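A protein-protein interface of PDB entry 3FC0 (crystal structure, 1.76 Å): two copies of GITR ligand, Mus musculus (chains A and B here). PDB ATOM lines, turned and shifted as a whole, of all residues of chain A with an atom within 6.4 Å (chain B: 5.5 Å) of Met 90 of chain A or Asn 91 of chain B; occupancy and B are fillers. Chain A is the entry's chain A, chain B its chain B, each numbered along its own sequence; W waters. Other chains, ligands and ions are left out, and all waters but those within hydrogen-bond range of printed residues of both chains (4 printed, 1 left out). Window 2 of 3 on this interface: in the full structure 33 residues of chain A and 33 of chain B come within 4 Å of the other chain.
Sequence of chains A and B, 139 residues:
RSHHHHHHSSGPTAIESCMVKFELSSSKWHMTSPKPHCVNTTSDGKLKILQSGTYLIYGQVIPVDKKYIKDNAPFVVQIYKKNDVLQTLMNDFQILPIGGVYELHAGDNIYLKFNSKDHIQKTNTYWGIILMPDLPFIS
Met 90 of chain A touches Asn 91 of chain B, and with the chains exchanged Asn 91 of chain A touches Met 90 of chain B.
Met 90 of chain A touches Gln 94 of chain B, and with the chains exchanged Gln 94 of chain A touches Met 90 of chain B.
8 positions are printed for both chains.
The backbone carbonyl oxygen of Met 90 of chain A sits at hydrogen-bond distance from the side-chain amide nitrogen of Gln 94 of chain B, at 3.5 Å.
Along chain B the printed residues that touch a printed residue of chain A span positions 90 to 94.
Printed residues of chain A that touch a printed residue of chain B: Met 90, Asn 91 and Gln 94.
Along chain A the printed residues that touch a printed residue of chain B span positions 90 to 94.
Among the printed residues, 4 pairs touch across the chains.
Among the printed residues, no Asp or Glu carboxylate lies within 4 Å of a Lys or Arg side-chain nitrogen of the other chain.
Water W1 lies within hydrogen-bond range of the backbone NH (N) of Asp 92 of chain A, the side-chain amide nitrogen (NE2) of Gln 94 of chain A and the backbone carbonyl oxygen (O) of Met 90 of chain B.
Water W3 bridges NE2 of Gln 94 of chain B (2.9 Å) and N of Met 90 of chain A (2.9 Å).
Water W2 bridges the backbone carbonyl oxygen (O) of Met 90 of chain A (2.9 Å) and the side-chain amide nitrogen (ND2) of Asn 91 of chain B (3.0 Å).
Water W4 lies within hydrogen-bond range of N of Asp 92 of chain B (2.9 Å), NE2 of Gln 94 of chain B (3.0 Å) and O of Met 90 of chain A (3.3 Å).
Of the printed residues of chain B, Met 90 of chain A touches Asn 91 and Gln 94.
Printed residues of chain B within 4 Å of Asn 91 of chain A: Met 90.
Printed residues of chain A within 4 Å of Met 90 of chain B: Asn 91 (3.98 Å) and Gln 94 (3.6 Å).
Asn 91 of chain B touches just one residue of chain A: Met 90 (3.98 Å).
Of the printed residues of chain A, Gln 94 of chain B touches Met 90.
Among the printed residues, pairs that only touch across the chains: Met 90 of chain A with Asn 91 of chain B (3.98 Å), Asn 91 of chain A with Met 90 of chain B (3.98 Å) and Gln 94 of chain A with Met 90 of chain B (3.6 Å).
The side-chain amide oxygen of Asn 91 of chain B sits at hydrogen-bond distance from the backbone NH of Phe 93 of chain B (3.1 Å).
The side-chain amide oxygen (OD1) of Asn 91 of chain A lies within hydrogen-bond range of the backbone NH (N) of Gln 94 of chain A (2.9 Å).
The backbone NH (N) of Gln 94 of chain B lies within hydrogen-bond range of the side-chain amide oxygen (OD1) of Asn 91 of chain B.
The backbone carbonyl oxygen of Phe 75 of chain B is in hydrogen-bond range of the backbone NH of Asn 91 of chain B, 3.3 Å away.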
ATOM      1  N   PRO A  74       6.547 -13.041  27.852  1.00  0.00           N
ATOM      2  CA  PRO A  74       6.560 -12.099  26.731  1.00  0.00           C
ATOM      3  C   PRO A  74       5.510 -12.401  25.636  1.00  0.00           C
ATOM      4  O   PRO A  74       5.041 -13.523  25.527  1.00  0.00           O
ATOM      5  CB  PRO A  74       7.962 -12.292  26.140  1.00  0.00           C
ATOM      6  CG  PRO A  74       8.313 -13.717  26.477  1.00  0.00           C
ATOM      7  CD  PRO A  74       7.741 -13.901  27.881  1.00  0.00           C
ATOM      8  N   PHE A  75       5.155 -11.375  24.863  1.00  0.00           N
ATOM      9  CA  PHE A  75       4.215 -11.522  23.753  1.00  0.00           C
ATOM     10  C   PHE A  75       5.041 -11.930  22.512  1.00  0.00           C
ATOM     11  O   PHE A  75       5.769 -11.106  21.950  1.00  0.00           O
ATOM     12  CB  PHE A  75       3.488 -10.192  23.522  1.00  0.00           C
ATOM     13  CG  PHE A  75       2.581 -10.175  22.294  1.00  0.00           C
ATOM     14  CD1 PHE A  75       1.613 -11.158  22.081  1.00  0.00           C
ATOM     15  CD2 PHE A  75       2.713  -9.164  21.370  1.00  0.00           C
ATOM     16  CE1 PHE A  75       0.798 -11.116  20.942  1.00  0.00           C
ATOM     17  CE2 PHE A  75       1.895  -9.094  20.248  1.00  0.00           C
ATOM     18  CZ  PHE A  75       0.951 -10.072  20.020  1.00  0.00           C
ATOM     19  N   VAL A  76       4.911 -13.182  22.099  1.00  0.00           N
ATOM     20  CA  VAL A  76       5.722 -13.729  21.004  1.00  0.00           C
ATOM     21  C   VAL A  76       4.821 -14.512  20.044  1.00  0.00           C
ATOM     22  O   VAL A  76       3.935 -15.289  20.456  1.00  0.00           O
ATOM     23  CB  VAL A  76       6.848 -14.644  21.491  1.00  0.00           C
ATOM     24  CG1 VAL A  76       7.710 -15.099  20.295  1.00  0.00           C
ATOM     25  CG2 VAL A  76       7.746 -13.924  22.493  1.00  0.00           C
ATOM     26  N   VAL A  77       5.036 -14.306  18.750  1.00  0.00           N
ATOM     27  CA  VAL A  77       4.281 -15.077  17.744  1.00  0.00           C
ATOM     28  C   VAL A  77       5.265 -15.646  16.768  1.00  0.00           C
ATOM     29  O   VAL A  77       6.178 -14.942  16.356  1.00  0.00           O
ATOM     30  CB  VAL A  77       3.301 -14.165  16.974  1.00  0.00           C
ATOM     31  CG1 VAL A  77       2.540 -14.970  15.921  1.00  0.00           C
ATOM     32  CG2 VAL A  77       2.315 -13.434  17.938  1.00  0.00           C
ATOM     33  N   THR A  88      10.082 -15.222  13.922  1.00  0.00           N
ATOM     34  CA  THR A  88       9.692 -15.084  15.331  1.00  0.00           C
ATOM     35  C   THR A  88       9.550 -13.614  15.617  1.00  0.00           C
ATOM     36  O   THR A  88      10.482 -12.880  15.374  1.00  0.00           O
ATOM     37  CB  THR A  88      10.810 -15.664  16.262  1.00  0.00           C
ATOM     38  OG1 THR A  88      10.942 -17.044  15.972  1.00  0.00           O
ATOM     39  CG2 THR A  88      10.400 -15.511  17.704  1.00  0.00           C
ATOM     40  N   LEU A  89       8.393 -13.198  16.130  1.00  0.00           N
ATOM     41  CA  LEU A  89       8.084 -11.809  16.328  1.00  0.00           C
ATOM     42  C   LEU A  89       7.804 -11.547  17.808  1.00  0.00           C
ATOM     43  O   LEU A  89       7.182 -12.371  18.473  1.00  0.00           O
ATOM     44  CB  LEU A  89       6.840 -11.473  15.518  1.00  0.00           C
ATOM     45  CG  LEU A  89       6.924 -11.849  14.017  1.00  0.00           C
ATOM     46  CD1 LEU A  89       5.614 -11.344  13.375  1.00  0.00           C
ATOM     47  CD2 LEU A  89       8.100 -11.168  13.369  1.00  0.00           C
ATOM     48  N   MET A  90       8.244 -10.395  18.296  1.00  0.00           N
ATOM     49  CA  MET A  90       7.892  -9.979  19.668  1.00  0.00           C
ATOM     50  C   MET A  90       7.773  -8.468  19.748  1.00  0.00           C
ATOM     51  O   MET A  90       8.433  -7.730  19.021  1.00  0.00           O
ATOM     52  CB  MET A  90       8.983 -10.470  20.622  1.00  0.00           C
ATOM     53  CG  MET A  90       8.926  -9.823  22.024  1.00  0.00           C
ATOM     54  SD  MET A  90      10.158 -10.667  23.066  1.00  0.00           S
ATOM     55  CE  MET A  90      11.656 -10.276  22.189  1.00  0.00           C
ATOM     56  N   ASN A  91       6.924  -7.993  20.633  1.00  0.00           N
ATOM     57  CA  ASN A  91       6.835  -6.567  20.881  1.00  0.00           C
ATOM     58  C   ASN A  91       6.177  -6.412  22.244  1.00  0.00           C
ATOM     59  O   ASN A  91       5.850  -7.424  22.834  1.00  0.00           O
ATOM     60  CB  ASN A  91       6.160  -5.816  19.728  1.00  0.00           C
ATOM     61  CG  ASN A  91       4.630  -5.926  19.700  1.00  0.00           C
ATOM     62  OD1 ASN A  91       3.964  -6.326  20.683  1.00  0.00           O
ATOM     63  ND2 ASN A  91       4.047  -5.507  18.557  1.00  0.00           N
ATOM     64  N   ASP A  92       5.985  -5.180  22.735  1.00  0.00           N
ATOM     65  CA  ASP A  92       5.431  -4.981  24.079  1.00  0.00           C
ATOM     66  C   ASP A  92       3.916  -4.850  24.072  1.00  0.00           C
ATOM     67  O   ASP A  92       3.353  -3.796  24.444  1.00  0.00           O
ATOM     68  CB  ASP A  92       6.057  -3.715  24.685  1.00  0.00           C
ATOM     69  CG  ASP A  92       5.784  -3.565  26.151  1.00  0.00           C
ATOM     70  OD1 ASP A  92       5.480  -4.571  26.815  1.00  0.00           O
ATOM     71  OD2 ASP A  92       5.927  -2.411  26.631  1.00  0.00           O
ATOM     72  N   GLN A  94       1.698  -4.833  21.566  1.00  0.00           N
ATOM     73  CA  GLN A  94       1.116  -3.879  20.614  1.00  0.00           C
ATOM     74  C   GLN A  94       0.614  -4.655  19.384  1.00  0.00           C
ATOM     75  O   GLN A  94       1.006  -5.789  19.173  1.00  0.00           O
ATOM     76  CB  GLN A  94       2.144  -2.849  20.195  1.00  0.00           C
ATOM     77  CG  GLN A  94       2.696  -1.996  21.349  1.00  0.00           C
ATOM     78  CD  GLN A  94       3.921  -1.211  20.929  1.00  0.00           C
ATOM     79  OE1 GLN A  94       4.311  -0.244  21.593  1.00  0.00           O
ATOM     80  NE2 GLN A  94       4.521  -1.598  19.802  1.00  0.00           N
ATOM     81  N   LEU A  96       0.448  -6.388  16.038  1.00  0.00           N
ATOM     82  CA  LEU A  96       1.598  -7.048  15.436  1.00  0.00           C
ATOM     83  C   LEU A  96       1.263  -7.564  14.026  1.00  0.00           C
ATOM     84  O   LEU A  96       0.676  -8.647  13.876  1.00  0.00           O
ATOM     85  CB  LEU A  96       2.011  -8.251  16.267  1.00  0.00           C
ATOM     86  CG  LEU A  96       3.229  -9.051  15.862  1.00  0.00           C
ATOM     87  CD1 LEU A  96       4.563  -8.330  16.102  1.00  0.00           C
ATOM     88  CD2 LEU A  96       3.210 -10.381  16.628  1.00  0.00           C
ATOM     89  N   PRO B  74      14.962   4.340  19.854  1.00  0.00           N
ATOM     90  CA  PRO B  74      13.951   3.323  19.610  1.00  0.00           C
ATOM     91  C   PRO B  74      13.758   3.016  18.080  1.00  0.00           C
ATOM     92  O   PRO B  74      13.820   3.918  17.269  1.00  0.00           O
ATOM     93  CB  PRO B  74      12.696   3.929  20.253  1.00  0.00           C
ATOM     94  CG  PRO B  74      12.868   5.448  20.160  1.00  0.00           C
ATOM     95  CD  PRO B  74      14.385   5.705  19.950  1.00  0.00           C
ATOM     96  N   PHE B  75      13.556   1.750  17.719  1.00  0.00           N
ATOM     97  CA  PHE B  75      13.318   1.375  16.314  1.00  0.00           C
ATOM     98  C   PHE B  75      11.841   1.610  16.010  1.00  0.00           C
ATOM     99  O   PHE B  75      10.997   0.854  16.480  1.00  0.00           O
ATOM    100  CB  PHE B  75      13.683  -0.084  16.106  1.00  0.00           C
ATOM    101  CG  PHE B  75      13.618  -0.552  14.690  1.00  0.00           C
ATOM    102  CD1 PHE B  75      14.262   0.135  13.676  1.00  0.00           C
ATOM    103  CD2 PHE B  75      12.952  -1.725  14.372  1.00  0.00           C
ATOM    104  CE1 PHE B  75      14.223  -0.345  12.370  1.00  0.00           C
ATOM    105  CE2 PHE B  75      12.909  -2.184  13.089  1.00  0.00           C
ATOM    106  CZ  PHE B  75      13.546  -1.507  12.083  1.00  0.00           C
ATOM    107  N   LEU B  89       4.638   1.200  14.420  1.00  0.00           N
ATOM    108  CA  LEU B  89       5.285  -0.022  14.882  1.00  0.00           C
ATOM    109  C   LEU B  89       6.590   0.269  15.612  1.00  0.00           C
ATOM    110  O   LEU B  89       7.339   1.133  15.191  1.00  0.00           O
ATOM    111  CB  LEU B  89       5.618  -0.918  13.688  1.00  0.00           C
ATOM    112  CG  LEU B  89       4.432  -1.202  12.782  1.00  0.00           C
ATOM    113  CD1 LEU B  89       4.931  -2.137  11.654  1.00  0.00           C
ATOM    114  CD2 LEU B  89       3.238  -1.798  13.570  1.00  0.00           C
ATOM    115  N   MET B  90       6.865  -0.465  16.690  1.00  0.00           N
ATOM    116  CA  MET B  90       8.103  -0.272  17.451  1.00  0.00           C
ATOM    117  C   MET B  90       8.541  -1.595  17.991  1.00  0.00           C
ATOM    118  O   MET B  90       7.703  -2.400  18.390  1.00  0.00           O
ATOM    119  CB  MET B  90       7.873   0.651  18.672  1.00  0.00           C
ATOM    120  CG  MET B  90       6.915   1.770  18.460  1.00  0.00           C
ATOM    121  SD  MET B  90       6.932   2.834  19.951  1.00  0.00           S
ATOM    122  CE  MET B  90       8.511   2.284  20.621  1.00  0.00           C
ATOM    123  N   ASN B  91       9.850  -1.832  18.040  1.00  0.00           N
ATOM    124  CA  ASN B  91      10.365  -2.971  18.732  1.00  0.00           C
ATOM    125  C   ASN B  91      11.825  -2.744  19.053  1.00  0.00           C
ATOM    126  O   ASN B  91      12.379  -1.678  18.749  1.00  0.00           O
ATOM    127  CB  ASN B  91      10.129  -4.288  17.967  1.00  0.00           C
ATOM    128  CG  ASN B  91      10.958  -4.394  16.697  1.00  0.00           C
ATOM    129  OD1 ASN B  91      11.950  -3.702  16.554  1.00  0.00           O
ATOM    130  ND2 ASN B  91      10.559  -5.294  15.784  1.00  0.00           N
ATOM    131  N   ASP B  92      12.470  -3.735  19.650  1.00  0.00           N
ATOM    132  CA  ASP B  92      13.831  -3.505  20.080  1.00  0.00           C
ATOM    133  C   ASP B  92      14.796  -3.957  18.977  1.00  0.00           C
ATOM    134  O   ASP B  92      15.551  -4.913  19.130  1.00  0.00           O
ATOM    135  CB  ASP B  92      14.106  -4.246  21.403  1.00  0.00           C
ATOM    136  CG  ASP B  92      15.510  -3.987  21.948  1.00  0.00           C
ATOM    137  OD1 ASP B  92      16.078  -2.901  21.714  1.00  0.00           O
ATOM    138  OD2 ASP B  92      16.047  -4.894  22.617  1.00  0.00           O
ATOM    139  N   PHE B  93      14.751  -3.248  17.854  1.00  0.00           N
ATOM    140  CA  PHE B  93      15.687  -3.506  16.765  1.00  0.00           C
ATOM    141  C   PHE B  93      15.627  -4.953  16.280  1.00  0.00           C
ATOM    142  O   PHE B  93      16.621  -5.636  16.185  1.00  0.00           O
ATOM    143  CB  PHE B  93      17.100  -2.999  17.123  1.00  0.00           C
ATOM    144  CG  PHE B  93      17.154  -1.497  17.270  1.00  0.00           C
ATOM    145  CD1 PHE B  93      17.545  -0.698  16.213  1.00  0.00           C
ATOM    146  CD2 PHE B  93      16.768  -0.891  18.464  1.00  0.00           C
ATOM    147  CE1 PHE B  93      17.565   0.661  16.324  1.00  0.00           C
ATOM    148  CE2 PHE B  93      16.789   0.481  18.591  1.00  0.00           C
ATOM    149  CZ  PHE B  93      17.190   1.263  17.516  1.00  0.00           C
ATOM    150  N   GLN B  94      14.412  -5.406  15.941  1.00  0.00           N
ATOM    151  CA  GLN B  94      14.197  -6.760  15.392  1.00  0.00           C
ATOM    152  C   GLN B  94      13.420  -6.650  14.057  1.00  0.00           C
ATOM    153  O   GLN B  94      12.854  -5.613  13.783  1.00  0.00           O
ATOM    154  CB  GLN B  94      13.392  -7.614  16.385  1.00  0.00           C
ATOM    155  CG  GLN B  94      14.016  -7.579  17.799  1.00  0.00           C
ATOM    156  CD  GLN B  94      13.126  -8.169  18.908  1.00  0.00           C
ATOM    157  OE1 GLN B  94      13.614  -8.467  20.005  1.00  0.00           O
ATOM    158  NE2 GLN B  94      11.831  -8.344  18.630  1.00  0.00           N
ATOM    159  N   ILE B  95      13.463  -7.711  13.253  1.00  0.00           N
ATOM    160  CA  ILE B  95      12.684  -7.758  12.006  1.00  0.00           C
ATOM    161  C   ILE B  95      11.268  -7.274  12.269  1.00  0.00           C
ATOM    162  O   ILE B  95      10.593  -7.704  13.225  1.00  0.00           O
ATOM    163  CB  ILE B  95      12.664  -9.178  11.421  1.00  0.00           C
ATOM    164  CG1 ILE B  95      11.981  -9.160  10.037  1.00  0.00           C
ATOM    165  CG2 ILE B  95      11.906 -10.121  12.335  1.00  0.00           C
ATOM    166  CD1 ILE B  95      11.833 -10.566   9.387  1.00  0.00           C
ATOM    167  N   LEU B  96      10.789  -6.377  11.409  1.00  0.00           N
ATOM    168  CA  LEU B  96       9.481  -5.790  11.552  1.00  0.00           C
ATOM    169  C   LEU B  96       8.659  -5.947  10.245  1.00  0.00           C
ATOM    170  O   LEU B  96       8.833  -5.139   9.337  1.00  0.00           O
ATOM    171  CB  LEU B  96       9.661  -4.309  11.792  1.00  0.00           C
ATOM    172  CG  LEU B  96       8.579  -3.425  12.372  1.00  0.00           C
ATOM    173  CD1 LEU B  96       8.072  -4.023  13.689  1.00  0.00           C
ATOM    174  CD2 LEU B  96       9.192  -2.026  12.629  1.00  0.00           C
HETATM  175  O   HOH W   1       6.828  -2.834  21.324  1.00  0.00           O
HETATM  176  O   HOH W   2       7.836  -6.366  16.516  1.00  0.00           O
HETATM  177  O   HOH W   3      10.072  -9.035  16.432  1.00  0.00           O
HETATM  178  O   HOH W   4      10.968  -6.122  20.483  1.00  0.00           O
